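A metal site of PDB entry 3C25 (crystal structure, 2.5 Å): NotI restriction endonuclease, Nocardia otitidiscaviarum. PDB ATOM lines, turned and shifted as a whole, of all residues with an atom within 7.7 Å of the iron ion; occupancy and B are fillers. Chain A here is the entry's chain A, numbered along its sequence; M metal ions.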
ATOM      1  N   PHE A  19     -18.188 -29.821 -18.400  1.00  0.00           N
ATOM      2  CA  PHE A  19     -19.183 -28.740 -18.343  1.00  0.00           C
ATOM      3  C   PHE A  19     -20.625 -29.258 -18.254  1.00  0.00           C
ATOM      4  O   PHE A  19     -21.515 -28.795 -18.977  1.00  0.00           O
ATOM      5  CB  PHE A  19     -18.996 -27.755 -19.513  1.00  0.00           C
ATOM      6  CG  PHE A  19     -17.683 -27.041 -19.493  1.00  0.00           C
ATOM      7  CD1 PHE A  19     -17.479 -25.926 -18.678  1.00  0.00           C
ATOM      8  CD2 PHE A  19     -16.621 -27.480 -20.294  1.00  0.00           C
ATOM      9  CE1 PHE A  19     -16.249 -25.270 -18.656  1.00  0.00           C
ATOM     10  CE2 PHE A  19     -15.391 -26.824 -20.273  1.00  0.00           C
ATOM     11  CZ  PHE A  19     -15.207 -25.718 -19.461  1.00  0.00           C
ATOM     12  N   GLY A  20     -20.828 -30.237 -17.373  1.00  0.00           N
ATOM     13  CA  GLY A  20     -22.161 -30.756 -17.077  1.00  0.00           C
ATOM     14  C   GLY A  20     -22.635 -31.911 -17.935  1.00  0.00           C
ATOM     15  O   GLY A  20     -23.696 -32.494 -17.669  1.00  0.00           O
ATOM     16  N   THR A  41     -19.358 -23.084 -20.193  1.00  0.00           N
ATOM     17  CA  THR A  41     -20.460 -22.666 -19.324  1.00  0.00           C
ATOM     18  C   THR A  41     -20.909 -23.809 -18.396  1.00  0.00           C
ATOM     19  O   THR A  41     -21.233 -24.884 -18.888  1.00  0.00           O
ATOM     20  CB  THR A  41     -21.651 -22.196 -20.208  1.00  0.00           C
ATOM     21  OG1 THR A  41     -21.276 -21.019 -20.950  1.00  0.00           O
ATOM     22  CG2 THR A  41     -22.902 -21.908 -19.397  1.00  0.00           C
ATOM     23  N   CYS A  42     -20.919 -23.579 -17.070  1.00  0.00           N
ATOM     24  CA  CYS A  42     -21.607 -24.512 -16.149  1.00  0.00           C
ATOM     25  C   CYS A  42     -23.110 -24.288 -16.382  1.00  0.00           C
ATOM     26  O   CYS A  42     -23.628 -23.182 -16.163  1.00  0.00           O
ATOM     27  CB  CYS A  42     -21.210 -24.336 -14.650  1.00  0.00           C
ATOM     28  SG  CYS A  42     -20.126 -25.670 -13.803  1.00  0.00           S
ATOM     29  N   PRO A  43     -23.817 -25.318 -16.876  1.00  0.00           N
ATOM     30  CA  PRO A  43     -25.252 -25.221 -17.157  1.00  0.00           C
ATOM     31  C   PRO A  43     -26.106 -25.044 -15.897  1.00  0.00           C
ATOM     32  O   PRO A  43     -27.231 -24.566 -15.988  1.00  0.00           O
ATOM     33  CB  PRO A  43     -25.569 -26.552 -17.828  1.00  0.00           C
ATOM     34  CG  PRO A  43     -24.529 -27.487 -17.334  1.00  0.00           C
ATOM     35  CD  PRO A  43     -23.290 -26.661 -17.214  1.00  0.00           C
ATOM     36  N   PHE A  44     -25.562 -25.423 -14.755  1.00  0.00           N
ATOM     37  CA  PHE A  44     -26.302 -25.410 -13.486  1.00  0.00           C
ATOM     38  C   PHE A  44     -26.406 -24.008 -12.900  1.00  0.00           C
ATOM     39  O   PHE A  44     -27.447 -23.643 -12.357  1.00  0.00           O
ATOM     40  CB  PHE A  44     -25.667 -26.384 -12.491  1.00  0.00           C
ATOM     41  CG  PHE A  44     -25.207 -27.665 -13.121  1.00  0.00           C
ATOM     42  CD1 PHE A  44     -26.127 -28.635 -13.505  1.00  0.00           C
ATOM     43  CD2 PHE A  44     -23.857 -27.890 -13.355  1.00  0.00           C
ATOM     44  CE1 PHE A  44     -25.703 -29.815 -14.106  1.00  0.00           C
ATOM     45  CE2 PHE A  44     -23.425 -29.067 -13.950  1.00  0.00           C
ATOM     46  CZ  PHE A  44     -24.357 -30.031 -14.338  1.00  0.00           C
ATOM     47  N   LEU A  45     -25.329 -23.230 -13.015  1.00  0.00           N
ATOM     48  CA  LEU A  45     -25.356 -21.812 -12.640  1.00  0.00           C
ATOM     49  C   LEU A  45     -26.180 -20.990 -13.625  1.00  0.00           C
ATOM     50  O   LEU A  45     -26.883 -20.051 -13.229  1.00  0.00           O
ATOM     51  CB  LEU A  45     -23.936 -21.255 -12.512  1.00  0.00           C
ATOM     52  CG  LEU A  45     -23.158 -21.616 -11.246  1.00  0.00           C
ATOM     53  CD1 LEU A  45     -21.668 -21.408 -11.444  1.00  0.00           C
ATOM     54  CD2 LEU A  45     -23.672 -20.825 -10.063  1.00  0.00           C
ATOM     55  N   SER A  54     -19.968 -18.983 -16.894  1.00  0.00           N
ATOM     56  CA  SER A  54     -18.864 -19.944 -17.069  1.00  0.00           C
ATOM     57  C   SER A  54     -18.566 -20.661 -15.753  1.00  0.00           C
ATOM     58  O   SER A  54     -18.912 -20.162 -14.679  1.00  0.00           O
ATOM     59  CB  SER A  54     -17.616 -19.237 -17.606  1.00  0.00           C
ATOM     60  OG  SER A  54     -17.375 -18.003 -16.949  1.00  0.00           O
ATOM     61  N   CYS A  55     -17.928 -21.838 -15.829  1.00  0.00           N
ATOM     62  CA  CYS A  55     -17.513 -22.559 -14.611  1.00  0.00           C
ATOM     63  C   CYS A  55     -16.591 -21.663 -13.816  1.00  0.00           C
ATOM     64  O   CYS A  55     -15.862 -20.840 -14.385  1.00  0.00           O
ATOM     65  CB  CYS A  55     -16.845 -23.928 -14.910  1.00  0.00           C
ATOM     66  SG  CYS A  55     -17.247 -25.286 -13.689  1.00  0.00           S
ATOM     67  N   VAL A  56     -16.638 -21.804 -12.501  1.00  0.00           N
ATOM     68  CA  VAL A  56     -15.903 -20.942 -11.578  1.00  0.00           C
ATOM     69  C   VAL A  56     -14.440 -21.358 -11.408  1.00  0.00           C
ATOM     70  O   VAL A  56     -13.647 -20.640 -10.806  1.00  0.00           O
ATOM     71  CB  VAL A  56     -16.601 -20.871 -10.196  1.00  0.00           C
ATOM     72  CG1 VAL A  56     -18.025 -20.343 -10.340  1.00  0.00           C
ATOM     73  CG2 VAL A  56     -16.595 -22.240  -9.498  1.00  0.00           C
ATOM     74  N   LYS A  57     -14.095 -22.531 -11.950  1.00  0.00           N
ATOM     75  CA  LYS A  57     -12.821 -23.173 -11.646  1.00  0.00           C
ATOM     76  C   LYS A  57     -11.652 -22.603 -12.415  1.00  0.00           C
ATOM     77  O   LYS A  57     -11.822 -22.083 -13.509  1.00  0.00           O
ATOM     78  CB  LYS A  57     -12.910 -24.686 -11.884  1.00  0.00           C
ATOM     79  CG  LYS A  57     -13.863 -25.394 -10.939  1.00  0.00           C
ATOM     80  CD  LYS A  57     -13.778 -26.886 -11.133  1.00  0.00           C
ATOM     81  CE  LYS A  57     -14.435 -27.623  -9.991  1.00  0.00           C
ATOM     82  NZ  LYS A  57     -14.288 -29.089 -10.176  1.00  0.00           N
ATOM     83  N   SER A  61      -8.456 -27.149 -13.771  1.00  0.00           N
ATOM     84  CA  SER A  61      -9.587 -28.054 -13.597  1.00  0.00           C
ATOM     85  C   SER A  61     -10.892 -27.508 -14.162  1.00  0.00           C
ATOM     86  O   SER A  61     -11.974 -27.880 -13.696  1.00  0.00           O
ATOM     87  CB  SER A  61      -9.743 -28.427 -12.119  1.00  0.00           C
ATOM     88  OG  SER A  61     -10.077 -27.307 -11.336  1.00  0.00           O
ATOM     89  N   ARG A  62     -10.795 -26.654 -15.185  1.00  0.00           N
ATOM     90  CA  ARG A  62     -11.970 -25.991 -15.771  1.00  0.00           C
ATOM     91  C   ARG A  62     -12.932 -26.986 -16.412  1.00  0.00           C
ATOM     92  O   ARG A  62     -12.565 -27.738 -17.323  1.00  0.00           O
ATOM     93  CB  ARG A  62     -11.532 -24.932 -16.793  1.00  0.00           C
ATOM     94  CG  ARG A  62     -12.674 -24.142 -17.425  1.00  0.00           C
ATOM     95  CD  ARG A  62     -12.814 -22.746 -16.837  1.00  0.00           C
ATOM     96  NE  ARG A  62     -11.984 -21.788 -17.557  1.00  0.00           N
ATOM     97  CZ  ARG A  62     -10.949 -21.123 -17.033  1.00  0.00           C
ATOM     98  NH1 ARG A  62     -10.619 -21.282 -15.755  1.00  0.00           N
ATOM     99  NH2 ARG A  62     -10.251 -20.283 -17.783  1.00  0.00           N
ATOM    100  N   GLY A  63     -14.173 -27.007 -15.927  1.00  0.00           N
ATOM    101  CA  GLY A  63     -15.231 -27.839 -16.495  1.00  0.00           C
ATOM    102  C   GLY A  63     -15.275 -29.280 -16.006  1.00  0.00           C
ATOM    103  O   GLY A  63     -16.131 -30.051 -16.458  1.00  0.00           O
ATOM    104  N   VAL A  64     -14.363 -29.651 -15.116  1.00  0.00           N
ATOM    105  CA  VAL A  64     -14.358 -30.983 -14.525  1.00  0.00           C
ATOM    106  C   VAL A  64     -15.365 -31.015 -13.374  1.00  0.00           C
ATOM    107  O   VAL A  64     -15.015 -30.804 -12.205  1.00  0.00           O
ATOM    108  CB  VAL A  64     -12.937 -31.405 -14.035  1.00  0.00           C
ATOM    109  CG1 VAL A  64     -12.917 -32.865 -13.632  1.00  0.00           C
ATOM    110  CG2 VAL A  64     -11.910 -31.169 -15.115  1.00  0.00           C
ATOM    111  N   CYS A  65     -16.620 -31.270 -13.724  1.00  0.00           N
ATOM    112  CA  CYS A  65     -17.702 -31.245 -12.760  1.00  0.00           C
ATOM    113  C   CYS A  65     -17.856 -32.624 -12.080  1.00  0.00           C
ATOM    114  O   CYS A  65     -18.293 -32.709 -10.927  1.00  0.00           O
ATOM    115  CB  CYS A  65     -19.013 -30.686 -13.396  1.00  0.00           C
ATOM    116  SG  CYS A  65     -19.109 -28.790 -13.608  1.00  0.00           S
ATOM    117  N   VAL A  66     -17.451 -33.703 -12.767  1.00  0.00           N
ATOM    118  CA  VAL A  66     -17.527 -35.071 -12.225  1.00  0.00           C
ATOM    119  C   VAL A  66     -16.318 -35.926 -12.651  1.00  0.00           C
ATOM    120  O   VAL A  66     -15.861 -35.846 -13.796  1.00  0.00           O
ATOM    121  CB  VAL A  66     -18.845 -35.809 -12.630  1.00  0.00           C
ATOM    122  CG1 VAL A  66     -18.915 -37.211 -12.027  1.00  0.00           C
ATOM    123  CG2 VAL A  66     -20.087 -35.020 -12.217  1.00  0.00           C
ATOM    124  N   VAL A  80     -17.431 -33.231  -8.073  1.00  0.00           N
ATOM    125  CA  VAL A  80     -16.165 -32.587  -7.791  1.00  0.00           C
ATOM    126  C   VAL A  80     -16.289 -31.046  -7.780  1.00  0.00           C
ATOM    127  O   VAL A  80     -15.294 -30.327  -7.659  1.00  0.00           O
ATOM    128  CB  VAL A  80     -15.076 -33.141  -8.768  1.00  0.00           C
ATOM    129  CG1 VAL A  80     -14.064 -32.096  -9.187  1.00  0.00           C
ATOM    130  CG2 VAL A  80     -14.369 -34.340  -8.150  1.00  0.00           C
ATOM    131  N   CYS A  81     -17.528 -30.570  -7.885  1.00  0.00           N
ATOM    132  CA  CYS A  81     -17.877 -29.143  -7.952  1.00  0.00           C
ATOM    133  C   CYS A  81     -19.212 -29.009  -7.210  1.00  0.00           C
ATOM    134  O   CYS A  81     -20.178 -29.680  -7.576  1.00  0.00           O
ATOM    135  CB  CYS A  81     -17.993 -28.708  -9.439  1.00  0.00           C
ATOM    136  SG  CYS A  81     -18.465 -26.966  -9.930  1.00  0.00           S
ATOM    137  N   PRO A  82     -19.252 -28.199  -6.130  1.00  0.00           N
ATOM    138  CA  PRO A  82     -20.502 -27.973  -5.384  1.00  0.00           C
ATOM    139  C   PRO A  82     -21.647 -27.470  -6.277  1.00  0.00           C
ATOM    140  O   PRO A  82     -22.819 -27.757  -6.005  1.00  0.00           O
ATOM    141  CB  PRO A  82     -20.111 -26.879  -4.378  1.00  0.00           C
ATOM    142  CG  PRO A  82     -18.647 -27.063  -4.196  1.00  0.00           C
ATOM    143  CD  PRO A  82     -18.134 -27.446  -5.544  1.00  0.00           C
ATOM    144  N   ASN A  83     -21.291 -26.751  -7.333  1.00  0.00           N
ATOM    145  CA  ASN A  83     -22.253 -26.228  -8.302  1.00  0.00           C
ATOM    146  C   ASN A  83     -22.893 -27.322  -9.160  1.00  0.00           C
ATOM    147  O   ASN A  83     -23.962 -27.117  -9.734  1.00  0.00           O
ATOM    148  CB  ASN A  83     -21.587 -25.161  -9.172  1.00  0.00           C
ATOM    149  CG  ASN A  83     -20.954 -24.052  -8.347  1.00  0.00           C
ATOM    150  OD1 ASN A  83     -21.493 -23.650  -7.314  1.00  0.00           O
ATOM    151  ND2 ASN A  83     -19.816 -23.546  -8.805  1.00  0.00           N
ATOM    152  N   ARG A  84     -22.242 -28.480  -9.245  1.00  0.00           N
ATOM    153  CA  ARG A  84     -22.817 -29.657  -9.909  1.00  0.00           C
ATOM    154  C   ARG A  84     -24.027 -30.205  -9.127  1.00  0.00           C
ATOM    155  O   ARG A  84     -24.932 -30.799  -9.707  1.00  0.00           O
ATOM    156  CB  ARG A  84     -21.714 -30.719 -10.133  1.00  0.00           C
ATOM    157  CG  ARG A  84     -22.137 -32.121 -10.562  1.00  0.00           C
ATOM    158  CD  ARG A  84     -22.830 -32.203 -11.919  1.00  0.00           C
ATOM    159  NE  ARG A  84     -24.279 -32.084 -11.752  1.00  0.00           N
ATOM    160  CZ  ARG A  84     -25.189 -32.738 -12.463  1.00  0.00           C
ATOM    161  NH1 ARG A  84     -26.478 -32.521 -12.224  1.00  0.00           N
ATOM    162  NH2 ARG A  84     -24.836 -33.597 -13.420  1.00  0.00           N
HETATM  163 FE    FE M   1     -18.565 -26.797 -12.337  1.00  0.00          FE
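N of Val 80 lies within hydrogen-bond range of O of Cys 65 (3.0 Å).
Of the 22 residues printed, 4 come within 4 Å of the iron ion.
SG of Cys 81 binds the iron ion (2.4 Å).
The iron ion is bound by SG of Cys 55 (2.4 Å).
SG of Cys 42 is bound to the iron ion (2.4 Å).
The side-chain sulfur (SG) of Cys 65 binds the iron ion, at 2.4 Å.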
